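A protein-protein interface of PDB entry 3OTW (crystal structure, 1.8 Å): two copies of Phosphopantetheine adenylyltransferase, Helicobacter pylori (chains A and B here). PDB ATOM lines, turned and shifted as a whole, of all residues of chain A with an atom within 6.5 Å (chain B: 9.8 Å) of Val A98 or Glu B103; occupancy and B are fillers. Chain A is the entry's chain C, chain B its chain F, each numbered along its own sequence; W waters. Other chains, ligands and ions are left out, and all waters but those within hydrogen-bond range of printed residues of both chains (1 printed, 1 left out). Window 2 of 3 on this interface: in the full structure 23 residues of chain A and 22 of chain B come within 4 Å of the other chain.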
ATOM      1  N   LEU A  96      -1.168  18.797  22.970  1.00  0.00           N
ATOM      2  CA  LEU A  96      -1.116  17.376  22.679  1.00  0.00           C
ATOM      3  C   LEU A  96      -2.442  16.973  22.089  1.00  0.00           C
ATOM      4  O   LEU A  96      -3.479  17.052  22.779  1.00  0.00           O
ATOM      5  CB  LEU A  96      -0.865  16.598  23.933  1.00  0.00           C
ATOM      6  CG  LEU A  96       0.557  16.764  24.421  1.00  0.00           C
ATOM      7  CD1 LEU A  96       0.669  15.910  25.628  1.00  0.00           C
ATOM      8  CD2 LEU A  96       1.614  16.411  23.328  1.00  0.00           C
ATOM      9  N   ARG A  97      -2.397  16.585  20.817  1.00  0.00           N
ATOM     10  CA  ARG A  97      -3.586  16.038  20.133  1.00  0.00           C
ATOM     11  C   ARG A  97      -3.371  14.578  19.762  1.00  0.00           C
ATOM     12  O   ARG A  97      -2.333  13.956  20.012  1.00  0.00           O
ATOM     13  CB  ARG A  97      -3.920  16.771  18.825  1.00  0.00           C
ATOM     14  CG  ARG A  97      -3.846  18.238  18.722  1.00  0.00           C
ATOM     15  CD  ARG A  97      -3.552  18.538  17.272  1.00  0.00           C
ATOM     16  NE  ARG A  97      -2.117  18.461  17.040  1.00  0.00           N
ATOM     17  CZ  ARG A  97      -1.558  18.163  15.877  1.00  0.00           C
ATOM     18  NH1 ARG A  97      -0.245  18.121  15.773  1.00  0.00           N
ATOM     19  NH2 ARG A  97      -2.316  17.888  14.843  1.00  0.00           N
ATOM     20  N   VAL A  98      -4.397  14.020  19.124  1.00  0.00           N
ATOM     21  CA  VAL A  98      -4.383  12.615  18.775  1.00  0.00           C
ATOM     22  C   VAL A  98      -3.167  12.213  17.936  1.00  0.00           C
ATOM     23  O   VAL A  98      -2.570  11.139  18.194  1.00  0.00           O
ATOM     24  CB  VAL A  98      -5.686  12.255  17.983  1.00  0.00           C
ATOM     25  CG1 VAL A  98      -5.611  10.846  17.346  1.00  0.00           C
ATOM     26  CG2 VAL A  98      -6.896  12.359  18.890  1.00  0.00           C
ATOM     27  N   VAL A  99      -2.860  12.996  16.910  1.00  0.00           N
ATOM     28  CA  VAL A  99      -1.741  12.625  16.020  1.00  0.00           C
ATOM     29  C   VAL A  99      -0.422  13.223  16.474  1.00  0.00           C
ATOM     30  O   VAL A  99       0.582  13.166  15.718  1.00  0.00           O
ATOM     31  CB  VAL A  99      -1.976  12.934  14.487  1.00  0.00           C
ATOM     32  CG1 VAL A  99      -3.347  12.414  14.039  1.00  0.00           C
ATOM     33  CG2 VAL A  99      -1.774  14.436  14.172  1.00  0.00           C
ATOM     34  N   SER A 100      -0.387  13.784  17.697  1.00  0.00           N
ATOM     35  CA  SER A 100       0.901  14.310  18.168  1.00  0.00           C
ATOM     36  C   SER A 100       1.931  13.207  18.155  1.00  0.00           C
ATOM     37  O   SER A 100       1.603  12.032  18.398  1.00  0.00           O
ATOM     38  CB  SER A 100       0.800  14.932  19.562  1.00  0.00           C
ATOM     39  OG  SER A 100       0.037  16.104  19.463  1.00  0.00           O
ATOM     40  N   ASP A 101       3.183  13.574  17.855  1.00  0.00           N
ATOM     41  CA  ASP A 101       4.250  12.608  17.949  1.00  0.00           C
ATOM     42  C   ASP A 101       4.821  12.784  19.324  1.00  0.00           C
ATOM     43  O   ASP A 101       5.636  13.685  19.562  1.00  0.00           O
ATOM     44  CB  ASP A 101       5.340  12.862  16.920  1.00  0.00           C
ATOM     45  CG  ASP A 101       6.460  11.858  17.013  1.00  0.00           C
ATOM     46  OD1 ASP A 101       6.641  11.181  18.065  1.00  0.00           O
ATOM     47  OD2 ASP A 101       7.171  11.737  16.006  1.00  0.00           O
ATOM     48  N   PRO A 126      -6.440  20.049  23.501  1.00  0.00           N
ATOM     49  CA  PRO A 126      -7.576  20.793  22.953  1.00  0.00           C
ATOM     50  C   PRO A 126      -8.868  20.112  23.369  1.00  0.00           C
ATOM     51  O   PRO A 126      -8.833  19.050  24.024  1.00  0.00           O
ATOM     52  CB  PRO A 126      -7.391  20.666  21.443  1.00  0.00           C
ATOM     53  CG  PRO A 126      -6.795  19.234  21.298  1.00  0.00           C
ATOM     54  CD  PRO A 126      -5.849  19.125  22.506  1.00  0.00           C
ATOM     55  N   LEU A 128     -12.090  17.770  22.900  1.00  0.00           N
ATOM     56  CA  LEU A 128     -12.269  16.512  22.196  1.00  0.00           C
ATOM     57  C   LEU A 128     -12.613  16.707  20.710  1.00  0.00           C
ATOM     58  O   LEU A 128     -12.046  16.030  19.802  1.00  0.00           O
ATOM     59  CB  LEU A 128     -13.398  15.684  22.907  1.00  0.00           C
ATOM     60  CG  LEU A 128     -13.554  14.197  22.556  1.00  0.00           C
ATOM     61  CD1 LEU A 128     -14.557  13.553  23.512  1.00  0.00           C
ATOM     62  CD2 LEU A 128     -14.084  14.009  21.157  1.00  0.00           C
ATOM     63  N   ALA A 131      -9.620  17.354  18.628  1.00  0.00           N
ATOM     64  CA  ALA A 131      -8.443  16.544  18.922  1.00  0.00           C
ATOM     65  C   ALA A 131      -7.837  15.958  17.634  1.00  0.00           C
ATOM     66  O   ALA A 131      -6.712  15.527  17.672  1.00  0.00           O
ATOM     67  CB  ALA A 131      -8.740  15.427  19.928  1.00  0.00           C
ATOM     68  N   PHE A 132      -8.595  15.947  16.537  1.00  0.00           N
ATOM     69  CA  PHE A 132      -8.092  15.370  15.296  1.00  0.00           C
ATOM     70  C   PHE A 132      -7.905  16.452  14.224  1.00  0.00           C
ATOM     71  O   PHE A 132      -7.944  16.133  13.014  1.00  0.00           O
ATOM     72  CB  PHE A 132      -9.125  14.416  14.724  1.00  0.00           C
ATOM     73  CG  PHE A 132      -9.368  13.191  15.595  1.00  0.00           C
ATOM     74  CD1 PHE A 132     -10.296  13.239  16.633  1.00  0.00           C
ATOM     75  CD2 PHE A 132      -8.687  12.027  15.351  1.00  0.00           C
ATOM     76  CE1 PHE A 132     -10.506  12.090  17.435  1.00  0.00           C
ATOM     77  CE2 PHE A 132      -8.905  10.850  16.154  1.00  0.00           C
ATOM     78  CZ  PHE A 132      -9.830  10.915  17.176  1.00  0.00           C
ATOM     79  N   LEU B  96       4.499  13.132  31.934  1.00  0.00           N
ATOM     80  CA  LEU B  96       4.654  12.419  30.654  1.00  0.00           C
ATOM     81  C   LEU B  96       6.090  11.924  30.575  1.00  0.00           C
ATOM     82  O   LEU B  96       7.043  12.729  30.550  1.00  0.00           O
ATOM     83  CB  LEU B  96       4.367  13.326  29.478  1.00  0.00           C
ATOM     84  CG  LEU B  96       2.898  13.685  29.272  1.00  0.00           C
ATOM     85  CD1 LEU B  96       2.747  14.569  28.047  1.00  0.00           C
ATOM     86  CD2 LEU B  96       2.036  12.433  29.164  1.00  0.00           C
ATOM     87  N   ARG B  97       6.228  10.599  30.574  1.00  0.00           N
ATOM     88  CA  ARG B  97       7.523   9.932  30.522  1.00  0.00           C
ATOM     89  C   ARG B  97       7.585   9.161  29.225  1.00  0.00           C
ATOM     90  O   ARG B  97       6.617   9.095  28.474  1.00  0.00           O
ATOM     91  CB  ARG B  97       7.639   8.875  31.608  1.00  0.00           C
ATOM     92  CG  ARG B  97       7.711   9.321  33.016  1.00  0.00           C
ATOM     93  CD  ARG B  97       7.562   8.060  33.852  1.00  0.00           C
ATOM     94  NE  ARG B  97       6.185   7.554  33.781  1.00  0.00           N
ATOM     95  CZ  ARG B  97       5.825   6.287  33.935  1.00  0.00           C
ATOM     96  NH1 ARG B  97       4.543   5.956  33.866  1.00  0.00           N
ATOM     97  NH2 ARG B  97       6.730   5.348  34.142  1.00  0.00           N
ATOM     98  N   VAL B  99       7.639   5.969  28.597  1.00  0.00           N
ATOM     99  CA  VAL B  99       6.731   4.814  28.518  1.00  0.00           C
ATOM    100  C   VAL B  99       5.266   5.212  28.769  1.00  0.00           C
ATOM    101  O   VAL B  99       4.382   4.346  28.794  1.00  0.00           O
ATOM    102  CB  VAL B  99       7.147   3.615  29.463  1.00  0.00           C
ATOM    103  CG1 VAL B  99       8.595   3.214  29.191  1.00  0.00           C
ATOM    104  CG2 VAL B  99       6.961   3.979  30.960  1.00  0.00           C
ATOM    105  N   SER B 100       5.004   6.514  28.903  1.00  0.00           N
ATOM    106  CA  SER B 100       3.632   6.970  29.060  1.00  0.00           C
ATOM    107  C   SER B 100       2.774   6.497  27.898  1.00  0.00           C
ATOM    108  O   SER B 100       3.201   6.509  26.746  1.00  0.00           O
ATOM    109  CB  SER B 100       3.538   8.495  29.177  1.00  0.00           C
ATOM    110  OG  SER B 100       4.012   8.958  30.426  1.00  0.00           O
ATOM    111  N   ASP B 101       1.541   6.105  28.210  1.00  0.00           N
ATOM    112  CA  ASP B 101       0.591   5.721  27.177  1.00  0.00           C
ATOM    113  C   ASP B 101      -0.167   6.994  26.810  1.00  0.00           C
ATOM    114  O   ASP B 101      -1.153   7.403  27.464  1.00  0.00           O
ATOM    115  CB  ASP B 101      -0.333   4.625  27.693  1.00  0.00           C
ATOM    116  CG  ASP B 101      -1.363   4.201  26.671  1.00  0.00           C
ATOM    117  OD1 ASP B 101      -1.614   4.938  25.679  1.00  0.00           O
ATOM    118  OD2 ASP B 101      -1.924   3.102  26.868  1.00  0.00           O
ATOM    119  N   PHE B 102       0.333   7.618  25.765  1.00  0.00           N
ATOM    120  CA  PHE B 102      -0.090   8.959  25.380  1.00  0.00           C
ATOM    121  C   PHE B 102      -1.590   9.061  25.075  1.00  0.00           C
ATOM    122  O   PHE B 102      -2.300  10.030  25.482  1.00  0.00           O
ATOM    123  CB  PHE B 102       0.741   9.367  24.177  1.00  0.00           C
ATOM    124  CG  PHE B 102       0.282  10.608  23.524  1.00  0.00           C
ATOM    125  CD1 PHE B 102      -0.135  10.586  22.189  1.00  0.00           C
ATOM    126  CD2 PHE B 102       0.256  11.806  24.226  1.00  0.00           C
ATOM    127  CE1 PHE B 102      -0.582  11.724  21.566  1.00  0.00           C
ATOM    128  CE2 PHE B 102      -0.187  12.976  23.603  1.00  0.00           C
ATOM    129  CZ  PHE B 102      -0.605  12.926  22.265  1.00  0.00           C
ATOM    130  N   GLU B 103      -2.084   8.080  24.338  1.00  0.00           N
ATOM    131  CA  GLU B 103      -3.482   8.166  23.957  1.00  0.00           C
ATOM    132  C   GLU B 103      -4.350   7.851  25.183  1.00  0.00           C
ATOM    133  O   GLU B 103      -5.458   8.388  25.318  1.00  0.00           O
ATOM    134  CB  GLU B 103      -3.793   7.209  22.804  1.00  0.00           C
ATOM    135  CG  GLU B 103      -3.007   7.506  21.459  1.00  0.00           C
ATOM    136  CD  GLU B 103      -3.371   8.831  20.731  1.00  0.00           C
ATOM    137  OE1 GLU B 103      -2.679   9.157  19.743  1.00  0.00           O
ATOM    138  OE2 GLU B 103      -4.321   9.560  21.118  1.00  0.00           O
ATOM    139  N   TYR B 104      -3.873   6.971  26.057  1.00  0.00           N
ATOM    140  CA  TYR B 104      -4.575   6.699  27.333  1.00  0.00           C
ATOM    141  C   TYR B 104      -4.664   7.963  28.234  1.00  0.00           C
ATOM    142  O   TYR B 104      -5.668   8.211  28.928  1.00  0.00           O
ATOM    143  CB  TYR B 104      -3.878   5.577  28.089  1.00  0.00           C
ATOM    144  CG  TYR B 104      -4.111   5.570  29.587  1.00  0.00           C
ATOM    145  CD1 TYR B 104      -3.231   6.228  30.462  1.00  0.00           C
ATOM    146  CD2 TYR B 104      -5.222   4.923  30.137  1.00  0.00           C
ATOM    147  CE1 TYR B 104      -3.449   6.218  31.843  1.00  0.00           C
ATOM    148  CE2 TYR B 104      -5.446   4.915  31.507  1.00  0.00           C
ATOM    149  CZ  TYR B 104      -4.564   5.551  32.350  1.00  0.00           C
ATOM    150  OH  TYR B 104      -4.801   5.517  33.715  1.00  0.00           O
ATOM    151  N   GLU B 105      -3.597   8.750  28.241  1.00  0.00           N
ATOM    152  CA  GLU B 105      -3.641  10.038  28.961  1.00  0.00           C
ATOM    153  C   GLU B 105      -4.693  10.973  28.398  1.00  0.00           C
ATOM    154  O   GLU B 105      -5.448  11.573  29.155  1.00  0.00           O
ATOM    155  CB  GLU B 105      -2.270  10.721  28.957  1.00  0.00           C
ATOM    156  CG  GLU B 105      -1.268   9.958  29.801  1.00  0.00           C
ATOM    157  CD  GLU B 105      -1.477  10.104  31.282  1.00  0.00           C
ATOM    158  OE1 GLU B 105      -2.222  10.995  31.741  1.00  0.00           O
ATOM    159  OE2 GLU B 105      -0.886   9.296  32.016  1.00  0.00           O
ATOM    160  N   LEU B 106      -4.788  11.061  27.078  1.00  0.00           N
ATOM    161  CA  LEU B 106      -5.784  11.937  26.457  1.00  0.00           C
ATOM    162  C   LEU B 106      -7.175  11.407  26.824  1.00  0.00           C
ATOM    163  O   LEU B 106      -8.075  12.162  27.214  1.00  0.00           O
ATOM    164  CB  LEU B 106      -5.611  11.968  24.933  1.00  0.00           C
ATOM    165  CG  LEU B 106      -4.283  12.560  24.425  1.00  0.00           C
ATOM    166  CD1 LEU B 106      -4.297  12.534  22.884  1.00  0.00           C
ATOM    167  CD2 LEU B 106      -3.965  13.974  24.985  1.00  0.00           C
ATOM    168  N   GLN B 107      -7.324  10.087  26.751  1.00  0.00           N
ATOM    169  CA  GLN B 107      -8.599   9.427  27.109  1.00  0.00           C
ATOM    170  C   GLN B 107      -9.080   9.737  28.541  1.00  0.00           C
ATOM    171  O   GLN B 107     -10.258  10.085  28.786  1.00  0.00           O
ATOM    172  CB  GLN B 107      -8.416   7.923  26.988  1.00  0.00           C
ATOM    173  CG  GLN B 107      -9.634   7.134  27.471  1.00  0.00           C
ATOM    174  CD  GLN B 107      -9.462   5.607  27.348  1.00  0.00           C
ATOM    175  OE1 GLN B 107     -10.222   4.944  26.682  1.00  0.00           O
ATOM    176  NE2 GLN B 107      -8.434   5.075  27.979  1.00  0.00           N
ATOM    177  N   MET B 108      -8.171   9.589  29.477  1.00  0.00           N
ATOM    178  CA  MET B 108      -8.487   9.887  30.882  1.00  0.00           C
ATOM    179  C   MET B 108      -8.755  11.369  31.106  1.00  0.00           C
ATOM    180  O   MET B 108      -9.642  11.727  31.890  1.00  0.00           O
ATOM    181  CB  MET B 108      -7.329   9.440  31.774  1.00  0.00           C
ATOM    182  CG  MET B 108      -7.657   9.549  33.262  1.00  0.00           C
ATOM    183  SD  MET B 108      -6.599   8.361  34.180  1.00  0.00           S
ATOM    184  CE  MET B 108      -5.040   9.209  33.954  1.00  0.00           C
ATOM    185  N   GLY B 109      -8.015  12.237  30.407  1.00  0.00           N
ATOM    186  CA  GLY B 109      -8.261  13.689  30.474  1.00  0.00           C
ATOM    187  C   GLY B 109      -9.679  14.015  30.027  1.00  0.00           C
ATOM    188  O   GLY B 109     -10.432  14.743  30.722  1.00  0.00           O
ATOM    189  N   TYR B 110     -10.065  13.461  28.874  1.00  0.00           N
ATOM    190  CA  TYR B 110     -11.445  13.619  28.405  1.00  0.00           C
ATOM    191  C   TYR B 110     -12.488  12.968  29.305  1.00  0.00           C
ATOM    192  O   TYR B 110     -13.554  13.535  29.474  1.00  0.00           O
ATOM    193  CB  TYR B 110     -11.603  13.178  26.932  1.00  0.00           C
ATOM    194  CG  TYR B 110     -10.804  14.094  25.980  1.00  0.00           C
ATOM    195  CD1 TYR B 110     -10.931  15.511  26.047  1.00  0.00           C
ATOM    196  CD2 TYR B 110      -9.964  13.545  25.007  1.00  0.00           C
ATOM    197  CE1 TYR B 110     -10.173  16.369  25.153  1.00  0.00           C
ATOM    198  CE2 TYR B 110      -9.230  14.384  24.117  1.00  0.00           C
ATOM    199  CZ  TYR B 110      -9.335  15.772  24.207  1.00  0.00           C
ATOM    200  OH  TYR B 110      -8.568  16.534  23.338  1.00  0.00           O
ATOM    201  N   ALA B 111     -12.150  11.846  29.933  1.00  0.00           N
ATOM    202  CA  ALA B 111     -13.097  11.200  30.854  1.00  0.00           C
ATOM    203  C   ALA B 111     -13.325  12.059  32.071  1.00  0.00           C
ATOM    204  O   ALA B 111     -14.454  12.222  32.490  1.00  0.00           O
ATOM    205  CB  ALA B 111     -12.633   9.817  31.281  1.00  0.00           C
ATOM    206  N   TYR B 123       0.170  18.667  31.469  1.00  0.00           N
ATOM    207  CA  TYR B 123       1.227  17.662  31.582  1.00  0.00           C
ATOM    208  C   TYR B 123       2.606  18.272  31.686  1.00  0.00           C
ATOM    209  O   TYR B 123       2.915  19.298  31.021  1.00  0.00           O
ATOM    210  CB  TYR B 123       1.236  16.781  30.339  1.00  0.00           C
ATOM    211  CG  TYR B 123      -0.079  16.085  30.102  1.00  0.00           C
ATOM    212  CD1 TYR B 123      -0.324  14.799  30.628  1.00  0.00           C
ATOM    213  CD2 TYR B 123      -1.077  16.703  29.368  1.00  0.00           C
ATOM    214  CE1 TYR B 123      -1.572  14.130  30.396  1.00  0.00           C
ATOM    215  CE2 TYR B 123      -2.308  16.047  29.126  1.00  0.00           C
ATOM    216  CZ  TYR B 123      -2.533  14.778  29.637  1.00  0.00           C
ATOM    217  OH  TYR B 123      -3.754  14.172  29.393  1.00  0.00           O
HETATM  218  O   HOH W   1      -6.120  15.541  22.426  1.00  0.00           O
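Of the printed residues of chain B, Leu A96 touches Leu B96 (3.5 Å), Phe B102 (3.7 Å) and Leu B106 (3.8 Å). Of the printed residues of chain B, Arg A97 touches Phe B102 (3.0 Å) and Leu B106 (3.8 Å). Val A98 touches just these residues of chain B: Phe B102 and Glu B103. No residue of chain B comes within 4 Å of Val A99. Ser A100 touches just one residue of chain B: Phe B102 (3.6 Å). Asp A101 touches none of the printed residues of chain B. Of the printed residues of chain B, Pro A126 touches Tyr B110 (2.6 Å). Of the printed residues of chain B, Leu A128 touches Tyr B110. Ala A131 touches just one residue of chain B: Tyr B110 (3.6 Å). Tyr B104 touches none of the printed residues of chain A. Printed residues of chain A within 4 Å of Leu B106: Leu A96 and Arg A97. The nearest residue of chain A that does not touch Glu B103 is Val A99 (4.8 Å). The nearest printed residue of chain B that does not touch Leu A128 is Ala B111 (7.1 Å).
The side-chain carboxylate of Glu B103 lies close to the backbone carbonyl oxygen of Val A98 (2.5 Å). The side-chain hydroxyl (OH) of Tyr B110 sits at hydrogen-bond distance from the backbone carbonyl oxygen (O) of Pro A126, at 2.6 Å.
Leu A96 touches Leu B96 (CD1 to CD1, 3.5 Å). Leu A96 touches Phe B102. Leu B106 touches Leu A96 (CD2 to O, 3.8 Å). Arg A97 touches Phe B102. Leu B106 touches Arg A97. Phe B102 touches Val A98 (CE1 to O, 3.96 Å). Ser A100 touches Phe B102 (CB to CZ, 3.6 Å). Tyr B110 touches Leu A128 (CE1 to N, 3.3 Å). Ala A131 touches Tyr B110 (CB to OH, 3.6 Å).
The backbone carbonyl oxygen of Ala A131 lies within hydrogen-bond range of the backbone NH of Val A98 (3.1 Å). N of Glu B103 lies close to OD1 of Asp B101 (3.4 Å). N of Arg A97 lies within hydrogen-bond range of OG of Ser A100, 2.8 Å away.
Water W1 lies within hydrogen-bond range of the side-chain hydroxyl (OH) of Tyr B110 and the backbone carbonyl oxygen (O) of Leu A96.
Leu A96 touches its own counterpart, Leu B96. 5 positions are printed for both chains. Of the 11 pairs that touch across the chains among the printed residues, 1 has its exchanged pair printed and touching as well.
Hydrophobic or aromatic side chains of chain A within 4 Å of the printed part of chain B: Leu A96, Pro A126, Leu A128 and Ala A131. Printed residues of chain B that touch a printed residue of chain A: Leu B96, Phe B102, Glu B103, Leu B106 and Tyr B110. Hydrophobic or aromatic side chains of chain B within 4 Å of the printed part of chain A: Leu B96, Phe B102, Leu B106 and Tyr B110. Along chain B the printed residues that touch a printed residue of chain A span positions 96 to 110. Among the printed residues, 11 pairs touch across the chains.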
